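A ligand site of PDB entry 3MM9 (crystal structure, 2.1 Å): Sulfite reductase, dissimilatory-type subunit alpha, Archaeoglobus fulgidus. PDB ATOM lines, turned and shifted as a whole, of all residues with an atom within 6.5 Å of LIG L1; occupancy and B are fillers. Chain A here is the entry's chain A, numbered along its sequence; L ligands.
Merely in contact with LIG L1: Asp 223 and Phe 184.
Hydrophobic or aromatic side chains within 4 Å of LIG L1: Phe 184 and Ala 185.
SG of Cys 220 lies close to N of Asn 222 (3.6 Å).
SG of Cys 176 lies close to N of Gly 219.
The backbone NH of Gly 178 sits close to the side-chain sulfur of Cys 176.
The side-chain hydroxyl of Thr 189 is in hydrogen-bond range of the backbone carbonyl oxygen of Cys 176 (2.7 Å).
N of Cys 176 lies within hydrogen-bond range of O of Cys 217, 3.0 Å away.
O of Gly 219 lies within hydrogen-bond range of N of Cys 186 (2.7 Å).
The side-chain amide nitrogen of Asn 294 sits at hydrogen-bond distance from the side-chain amide oxygen of Asn 222 (2.9 Å).
The backbone carbonyl oxygen (O) of Phe 184 is in hydrogen-bond range of the side-chain sulfur (SG) of Cys 186 (3.6 Å).
SG of Cys 182 is bound to FE3 of LIG L1, 2.2 Å away.
S3 of LIG L1 lies close to N of Cys 224 (3.4 Å).
An iron atom (FE2) of LIG L1 is bound by the side-chain sulfur (SG) of Cys 224 (2.3 Å).
S3 of LIG L1 lies close to N of Cys 220 (3.7 Å).
The side-chain sulfur of Cys 220 is bound to an iron atom (FE1) of LIG L1 (2.3 Å).
An iron atom (FE4) of LIG L1 is bound by the side-chain sulfur (SG) of Cys 176 (2.4 Å).
N of Ala 185 lies close to S2 of LIG L1 (3.6 Å).
N of Gly 219 lies close to S3 of LIG L1 (3.7 Å).
The side-chain amide nitrogen (ND2) of Asn 222 sits close to a sulfur (S4) of LIG L1 (3.7 Å).
SG of Cys 182 lies close to O2 of LG2 L2 (3.7 Å).
FE1 of LG2 L2 is bound by SG of Cys 224 (2.4 Å).
O5 of LG2 L2 sits at hydrogen-bond distance from N of Met 177, at 2.8 Å.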
ATOM      1  N   CYS A 176     -34.445 -25.833  -6.998  1.00  0.00           N
ATOM      2  CA  CYS A 176     -33.880 -26.653  -8.085  1.00  0.00           C
ATOM      3  C   CYS A 176     -34.407 -28.088  -7.883  1.00  0.00           C
ATOM      4  O   CYS A 176     -34.831 -28.435  -6.789  1.00  0.00           O
ATOM      5  CB  CYS A 176     -32.349 -26.615  -8.021  1.00  0.00           C
ATOM      6  SG  CYS A 176     -31.758 -27.720  -6.787  1.00  0.00           S
ATOM      7  N   MET A 177     -34.367 -28.907  -8.930  1.00  0.00           N
ATOM      8  CA  MET A 177     -34.832 -30.296  -8.869  1.00  0.00           C
ATOM      9  C   MET A 177     -34.267 -31.083  -7.717  1.00  0.00           C
ATOM     10  O   MET A 177     -34.866 -32.056  -7.295  1.00  0.00           O
ATOM     11  CB  MET A 177     -34.508 -31.050 -10.185  1.00  0.00           C
ATOM     12  CG  MET A 177     -33.030 -31.293 -10.452  1.00  0.00           C
ATOM     13  SD  MET A 177     -32.642 -31.678 -12.197  1.00  0.00           S
ATOM     14  CE  MET A 177     -30.864 -32.088 -12.111  1.00  0.00           C
ATOM     15  N   GLY A 178     -33.077 -30.723  -7.257  1.00  0.00           N
ATOM     16  CA  GLY A 178     -32.506 -31.332  -6.091  1.00  0.00           C
ATOM     17  C   GLY A 178     -32.447 -32.865  -6.126  1.00  0.00           C
ATOM     18  O   GLY A 178     -32.242 -33.437  -7.178  1.00  0.00           O
ATOM     19  N   PRO A 179     -32.630 -33.515  -4.966  1.00  0.00           N
ATOM     20  CA  PRO A 179     -32.605 -34.980  -4.861  1.00  0.00           C
ATOM     21  C   PRO A 179     -33.587 -35.745  -5.774  1.00  0.00           C
ATOM     22  O   PRO A 179     -33.414 -36.945  -5.952  1.00  0.00           O
ATOM     23  CB  PRO A 179     -32.915 -35.268  -3.371  1.00  0.00           C
ATOM     24  CG  PRO A 179     -33.373 -34.003  -2.792  1.00  0.00           C
ATOM     25  CD  PRO A 179     -33.147 -32.854  -3.747  1.00  0.00           C
ATOM     26  N   CYS A 182     -30.939 -35.232  -9.014  1.00  0.00           N
ATOM     27  CA  CYS A 182     -29.545 -34.723  -8.975  1.00  0.00           C
ATOM     28  C   CYS A 182     -28.695 -35.388  -7.930  1.00  0.00           C
ATOM     29  O   CYS A 182     -29.007 -35.333  -6.722  1.00  0.00           O
ATOM     30  CB  CYS A 182     -29.511 -33.188  -8.783  1.00  0.00           C
ATOM     31  SG  CYS A 182     -27.863 -32.474  -9.109  1.00  0.00           S
ATOM     32  N   GLU A 183     -27.593 -35.995  -8.364  1.00  0.00           N
ATOM     33  CA  GLU A 183     -26.669 -36.630  -7.438  1.00  0.00           C
ATOM     34  C   GLU A 183     -25.774 -35.651  -6.653  1.00  0.00           C
ATOM     35  O   GLU A 183     -25.001 -36.083  -5.759  1.00  0.00           O
ATOM     36  CB  GLU A 183     -25.873 -37.751  -8.127  1.00  0.00           C
ATOM     37  CG  GLU A 183     -24.710 -37.301  -9.045  1.00  0.00           C
ATOM     38  CD  GLU A 183     -25.129 -36.853 -10.452  1.00  0.00           C
ATOM     39  OE1 GLU A 183     -26.321 -36.485 -10.684  1.00  0.00           O
ATOM     40  OE2 GLU A 183     -24.223 -36.818 -11.333  1.00  0.00           O
ATOM     41  N   PHE A 184     -25.835 -34.362  -6.970  1.00  0.00           N
ATOM     42  CA  PHE A 184     -25.064 -33.356  -6.181  1.00  0.00           C
ATOM     43  C   PHE A 184     -25.889 -32.757  -5.027  1.00  0.00           C
ATOM     44  O   PHE A 184     -25.343 -32.097  -4.159  1.00  0.00           O
ATOM     45  CB  PHE A 184     -24.552 -32.168  -7.044  1.00  0.00           C
ATOM     46  CG  PHE A 184     -23.725 -32.557  -8.253  1.00  0.00           C
ATOM     47  CD1 PHE A 184     -23.132 -33.824  -8.357  1.00  0.00           C
ATOM     48  CD2 PHE A 184     -23.513 -31.636  -9.270  1.00  0.00           C
ATOM     49  CE1 PHE A 184     -22.381 -34.151  -9.506  1.00  0.00           C
ATOM     50  CE2 PHE A 184     -22.811 -31.945 -10.409  1.00  0.00           C
ATOM     51  CZ  PHE A 184     -22.210 -33.205 -10.530  1.00  0.00           C
ATOM     52  N   ALA A 185     -27.207 -32.919  -5.036  1.00  0.00           N
ATOM     53  CA  ALA A 185     -28.025 -32.291  -3.972  1.00  0.00           C
ATOM     54  C   ALA A 185     -27.510 -32.445  -2.523  1.00  0.00           C
ATOM     55  O   ALA A 185     -27.279 -33.570  -2.044  1.00  0.00           O
ATOM     56  CB  ALA A 185     -29.477 -32.702  -4.091  1.00  0.00           C
ATOM     57  N   CYS A 186     -27.302 -31.345  -1.814  1.00  0.00           N
ATOM     58  CA  CYS A 186     -26.884 -31.479  -0.422  1.00  0.00           C
ATOM     59  C   CYS A 186     -28.020 -31.465   0.598  1.00  0.00           C
ATOM     60  O   CYS A 186     -27.771 -31.773   1.755  1.00  0.00           O
ATOM     61  CB  CYS A 186     -25.824 -30.442  -0.029  1.00  0.00           C
ATOM     62  SG  CYS A 186     -24.361 -30.618  -0.971  1.00  0.00           S
ATOM     63  N   THR A 189     -34.283 -30.021  -1.441  1.00  0.00           N
ATOM     64  CA  THR A 189     -34.697 -28.713  -1.904  1.00  0.00           C
ATOM     65  C   THR A 189     -36.202 -28.645  -2.088  1.00  0.00           C
ATOM     66  O   THR A 189     -36.848 -27.696  -1.611  1.00  0.00           O
ATOM     67  CB  THR A 189     -34.016 -28.281  -3.212  1.00  0.00           C
ATOM     68  OG1 THR A 189     -34.343 -29.223  -4.235  1.00  0.00           O
ATOM     69  CG2 THR A 189     -32.464 -28.200  -3.029  1.00  0.00           C
ATOM     70  N   CYS A 217     -34.336 -22.028  -3.177  1.00  0.00           N
ATOM     71  CA  CYS A 217     -33.656 -23.193  -2.589  1.00  0.00           C
ATOM     72  C   CYS A 217     -32.793 -23.907  -3.621  1.00  0.00           C
ATOM     73  O   CYS A 217     -33.327 -24.560  -4.539  1.00  0.00           O
ATOM     74  CB  CYS A 217     -34.679 -24.179  -1.984  1.00  0.00           C
ATOM     75  SG  CYS A 217     -35.823 -23.396  -0.803  1.00  0.00           S
ATOM     76  N   ALA A 218     -31.460 -23.807  -3.468  1.00  0.00           N
ATOM     77  CA  ALA A 218     -30.554 -24.516  -4.352  1.00  0.00           C
ATOM     78  C   ALA A 218     -29.821 -25.644  -3.645  1.00  0.00           C
ATOM     79  O   ALA A 218     -29.270 -25.440  -2.538  1.00  0.00           O
ATOM     80  CB  ALA A 218     -29.573 -23.554  -5.008  1.00  0.00           C
ATOM     81  N   GLY A 219     -29.728 -26.806  -4.307  1.00  0.00           N
ATOM     82  CA  GLY A 219     -29.280 -28.035  -3.590  1.00  0.00           C
ATOM     83  C   GLY A 219     -27.784 -28.018  -3.445  1.00  0.00           C
ATOM     84  O   GLY A 219     -27.222 -28.820  -2.695  1.00  0.00           O
ATOM     85  N   CYS A 220     -27.111 -27.141  -4.163  1.00  0.00           N
ATOM     86  CA  CYS A 220     -25.630 -27.146  -4.127  1.00  0.00           C
ATOM     87  C   CYS A 220     -25.140 -25.834  -4.718  1.00  0.00           C
ATOM     88  O   CYS A 220     -25.966 -25.086  -5.221  1.00  0.00           O
ATOM     89  CB  CYS A 220     -25.039 -28.384  -4.811  1.00  0.00           C
ATOM     90  SG  CYS A 220     -24.840 -28.258  -6.541  1.00  0.00           S
ATOM     91  N   PRO A 221     -23.819 -25.513  -4.564  1.00  0.00           N
ATOM     92  CA  PRO A 221     -23.281 -24.217  -4.967  1.00  0.00           C
ATOM     93  C   PRO A 221     -23.425 -23.896  -6.478  1.00  0.00           C
ATOM     94  O   PRO A 221     -23.283 -22.737  -6.864  1.00  0.00           O
ATOM     95  CB  PRO A 221     -21.791 -24.308  -4.578  1.00  0.00           C
ATOM     96  CG  PRO A 221     -21.744 -25.239  -3.429  1.00  0.00           C
ATOM     97  CD  PRO A 221     -22.810 -26.292  -3.808  1.00  0.00           C
ATOM     98  N   ASN A 222     -23.688 -24.891  -7.321  1.00  0.00           N
ATOM     99  CA  ASN A 222     -23.904 -24.565  -8.723  1.00  0.00           C
ATOM    100  C   ASN A 222     -25.081 -23.588  -8.848  1.00  0.00           C
ATOM    101  O   ASN A 222     -25.166 -22.862  -9.838  1.00  0.00           O
ATOM    102  CB  ASN A 222     -24.139 -25.787  -9.574  1.00  0.00           C
ATOM    103  CG  ASN A 222     -22.871 -26.571  -9.844  1.00  0.00           C
ATOM    104  OD1 ASN A 222     -21.810 -26.011 -10.044  1.00  0.00           O
ATOM    105  ND2 ASN A 222     -23.000 -27.893  -9.854  1.00  0.00           N
ATOM    106  N   ASP A 223     -25.982 -23.592  -7.860  1.00  0.00           N
ATOM    107  CA  ASP A 223     -27.073 -22.633  -7.734  1.00  0.00           C
ATOM    108  C   ASP A 223     -27.968 -22.613  -8.960  1.00  0.00           C
ATOM    109  O   ASP A 223     -28.140 -21.551  -9.612  1.00  0.00           O
ATOM    110  CB  ASP A 223     -26.566 -21.201  -7.459  1.00  0.00           C
ATOM    111  CG  ASP A 223     -27.652 -20.274  -6.811  1.00  0.00           C
ATOM    112  OD1 ASP A 223     -28.801 -20.709  -6.553  1.00  0.00           O
ATOM    113  OD2 ASP A 223     -27.359 -19.092  -6.588  1.00  0.00           O
ATOM    114  N   CYS A 224     -28.558 -23.758  -9.285  1.00  0.00           N
ATOM    115  CA  CYS A 224     -29.336 -23.826 -10.564  1.00  0.00           C
ATOM    116  C   CYS A 224     -30.711 -23.162 -10.527  1.00  0.00           C
ATOM    117  O   CYS A 224     -31.444 -23.203 -11.522  1.00  0.00           O
ATOM    118  CB  CYS A 224     -29.449 -25.286 -11.050  1.00  0.00           C
ATOM    119  SG  CYS A 224     -27.833 -26.129 -11.181  1.00  0.00           S
ATOM    120  N   VAL A 225     -31.103 -22.583  -9.379  1.00  0.00           N
ATOM    121  CA  VAL A 225     -32.245 -21.655  -9.357  1.00  0.00           C
ATOM    122  C   VAL A 225     -31.906 -20.194  -9.317  1.00  0.00           C
ATOM    123  O   VAL A 225     -32.836 -19.358  -9.170  1.00  0.00           O
ATOM    124  CB  VAL A 225     -33.186 -21.871  -8.157  1.00  0.00           C
ATOM    125  CG1 VAL A 225     -34.250 -22.819  -8.529  1.00  0.00           C
ATOM    126  CG2 VAL A 225     -32.441 -22.232  -6.922  1.00  0.00           C
ATOM    127  N   MET A 290     -17.600 -26.672  -6.546  1.00  0.00           N
ATOM    128  CA  MET A 290     -18.161 -27.752  -7.377  1.00  0.00           C
ATOM    129  C   MET A 290     -17.339 -28.164  -8.621  1.00  0.00           C
ATOM    130  O   MET A 290     -17.641 -29.216  -9.202  1.00  0.00           O
ATOM    131  CB  MET A 290     -19.632 -27.523  -7.751  1.00  0.00           C
ATOM    132  CG  MET A 290     -20.574 -27.470  -6.561  1.00  0.00           C
ATOM    133  SD  MET A 290     -20.634 -29.062  -5.721  1.00  0.00           S
ATOM    134  CE  MET A 290     -21.318 -30.050  -7.067  1.00  0.00           C
ATOM    135  N   ASN A 294     -18.329 -31.432 -10.746  1.00  0.00           N
ATOM    136  CA  ASN A 294     -18.935 -31.198 -12.029  1.00  0.00           C
ATOM    137  C   ASN A 294     -18.221 -31.949 -13.140  1.00  0.00           C
ATOM    138  O   ASN A 294     -18.869 -32.555 -14.007  1.00  0.00           O
ATOM    139  CB  ASN A 294     -18.955 -29.688 -12.345  1.00  0.00           C
ATOM    140  CG  ASN A 294     -19.870 -28.904 -11.401  1.00  0.00           C
ATOM    141  OD1 ASN A 294     -20.692 -29.501 -10.683  1.00  0.00           O
ATOM    142  ND2 ASN A 294     -19.794 -27.575 -11.446  1.00  0.00           N
HETATM  143 FE1  LIG L   1     -26.981 -28.473  -7.322  1.00  0.00          FE
HETATM  144 FE2  LIG L   1     -28.028 -27.765  -9.629  1.00  0.00          FE
HETATM  145 FE3  LIG L   1     -28.257 -30.308  -8.784  1.00  0.00          FE
HETATM  146 FE4  LIG L   1     -29.615 -28.379  -7.591  1.00  0.00          FE
HETATM  147  S1  LIG L   1     -29.756 -29.082  -9.680  1.00  0.00           S
HETATM  148  S2  LIG L   1     -28.472 -29.955  -6.617  1.00  0.00           S
HETATM  149  S3  LIG L   1     -28.178 -26.717  -7.669  1.00  0.00           S
HETATM  150  S4  LIG L   1     -26.471 -29.164  -9.344  1.00  0.00           S
HETATM  151 FE1  LG2 L   2     -27.522 -26.517 -13.553  1.00  0.00          FE
HETATM  152  C1  LG2 L   2     -24.867 -28.716 -13.595  1.00  0.00           C
HETATM  153  C2  LG2 L   2     -29.574 -29.081 -14.016  1.00  0.00           C
HETATM  154  C3  LG2 L   2     -30.060 -24.395 -14.360  1.00  0.00           C
HETATM  155  C4  LG2 L   2     -25.494 -23.944 -13.305  1.00  0.00           C
HETATM  156  N1  LG2 L   2     -27.308 -28.481 -13.679  1.00  0.00           N
HETATM  157  C5  LG2 L   2     -26.176 -29.223 -13.655  1.00  0.00           C
HETATM  158  C6  LG2 L   2     -26.365 -30.700 -13.682  1.00  0.00           C
HETATM  159  C7  LG2 L   2     -25.340 -31.415 -14.610  1.00  0.00           C
HETATM  160  C8  LG2 L   2     -26.252 -31.349 -12.302  1.00  0.00           C
HETATM  161  C9  LG2 L   2     -26.294 -32.853 -12.288  1.00  0.00           C
HETATM  162  O1  LG2 L   2     -27.239 -33.458 -12.866  1.00  0.00           O
HETATM  163  O2  LG2 L   2     -25.354 -33.386 -11.650  1.00  0.00           O
HETATM  164  C10 LG2 L   2     -27.801 -30.812 -14.140  1.00  0.00           C
HETATM  165  C11 LG2 L   2     -27.818 -31.161 -15.676  1.00  0.00           C
HETATM  166  C12 LG2 L   2     -27.450 -29.918 -16.567  1.00  0.00           C
HETATM  167  C13 LG2 L   2     -26.911 -30.203 -17.954  1.00  0.00           C
HETATM  168  O3  LG2 L   2     -27.648 -29.934 -18.954  1.00  0.00           O
HETATM  169  O4  LG2 L   2     -25.778 -30.742 -18.104  1.00  0.00           O
HETATM  170  C14 LG2 L   2     -28.219 -29.367 -13.983  1.00  0.00           C
HETATM  171  N2  LG2 L   2     -29.413 -26.753 -14.106  1.00  0.00           N
HETATM  172  C15 LG2 L   2     -30.108 -27.852 -14.133  1.00  0.00           C
HETATM  173  C16 LG2 L   2     -31.646 -27.726 -14.252  1.00  0.00           C
HETATM  174  C17 LG2 L   2     -32.414 -28.833 -14.986  1.00  0.00           C
HETATM  175  C18 LG2 L   2     -32.167 -27.544 -12.794  1.00  0.00           C
HETATM  176  C19 LG2 L   2     -33.678 -27.366 -12.544  1.00  0.00           C
HETATM  177  O5  LG2 L   2     -34.142 -27.554 -11.405  1.00  0.00           O
HETATM  178  O6  LG2 L   2     -34.426 -27.079 -13.473  1.00  0.00           O
HETATM  179  C20 LG2 L   2     -31.517 -26.358 -14.803  1.00  0.00           C
HETATM  180  C21 LG2 L   2     -32.032 -26.201 -16.228  1.00  0.00           C
HETATM  181  C22 LG2 L   2     -31.715 -25.002 -17.147  1.00  0.00           C
HETATM  182  C23 LG2 L   2     -32.042 -25.215 -18.601  1.00  0.00           C
HETATM  183  O7  LG2 L   2     -33.122 -25.752 -19.038  1.00  0.00           O
HETATM  184  O8  LG2 L   2     -31.197 -24.806 -19.419  1.00  0.00           O
HETATM  185  C24 LG2 L   2     -30.271 -25.722 -14.407  1.00  0.00           C
HETATM  186  N3  LG2 L   2     -27.713 -24.561 -13.767  1.00  0.00           N
HETATM  187  C25 LG2 L   2     -28.826 -23.900 -13.966  1.00  0.00           C
HETATM  188  C26 LG2 L   2     -28.671 -22.412 -13.891  1.00  0.00           C
HETATM  189  C27 LG2 L   2     -29.726 -21.423 -13.390  1.00  0.00           C
HETATM  190  C28 LG2 L   2     -29.878 -20.453 -14.556  1.00  0.00           C
HETATM  191  O9  LG2 L   2     -29.166 -20.530 -15.577  1.00  0.00           O
HETATM  192  O10 LG2 L   2     -30.702 -19.555 -14.478  1.00  0.00           O
HETATM  193  C29 LG2 L   2     -27.215 -22.238 -13.655  1.00  0.00           C
HETATM  194  C30 LG2 L   2     -26.614 -21.087 -12.825  1.00  0.00           C
HETATM  195  C31 LG2 L   2     -26.189 -20.192 -14.038  1.00  0.00           C
HETATM  196  C32 LG2 L   2     -24.864 -19.443 -13.852  1.00  0.00           C
HETATM  197  O11 LG2 L   2     -24.799 -18.292 -14.262  1.00  0.00           O
HETATM  198  O12 LG2 L   2     -23.846 -19.990 -13.361  1.00  0.00           O
HETATM  199  C33 LG2 L   2     -26.784 -23.677 -13.550  1.00  0.00           C
HETATM  200  N4  LG2 L   2     -25.605 -26.323 -13.365  1.00  0.00           N
HETATM  201  C34 LG2 L   2     -24.899 -25.164 -13.320  1.00  0.00           C
HETATM  202  C35 LG2 L   2     -23.380 -25.310 -13.183  1.00  0.00           C
HETATM  203  C36 LG2 L   2     -22.249 -24.325 -13.614  1.00  0.00           C
HETATM  204  C37 LG2 L   2     -21.633 -24.232 -15.003  1.00  0.00           C
HETATM  205  C38 LG2 L   2     -20.311 -23.477 -14.909  1.00  0.00           C
HETATM  206  O13 LG2 L   2     -19.362 -23.993 -15.525  1.00  0.00           O
HETATM  207  O14 LG2 L   2     -20.188 -22.369 -14.279  1.00  0.00           O
HETATM  208  C39 LG2 L   2     -23.256 -26.807 -13.291  1.00  0.00           C
HETATM  209  C40 LG2 L   2     -22.030 -27.631 -13.631  1.00  0.00           C
HETATM  210  C41 LG2 L   2     -21.843 -28.318 -14.945  1.00  0.00           C
HETATM  211  O15 LG2 L   2     -21.671 -27.602 -15.944  1.00  0.00           O
HETATM  212  O16 LG2 L   2     -21.771 -29.574 -14.969  1.00  0.00           O
HETATM  213  C42 LG2 L   2     -24.670 -27.317 -13.479  1.00  0.00           C
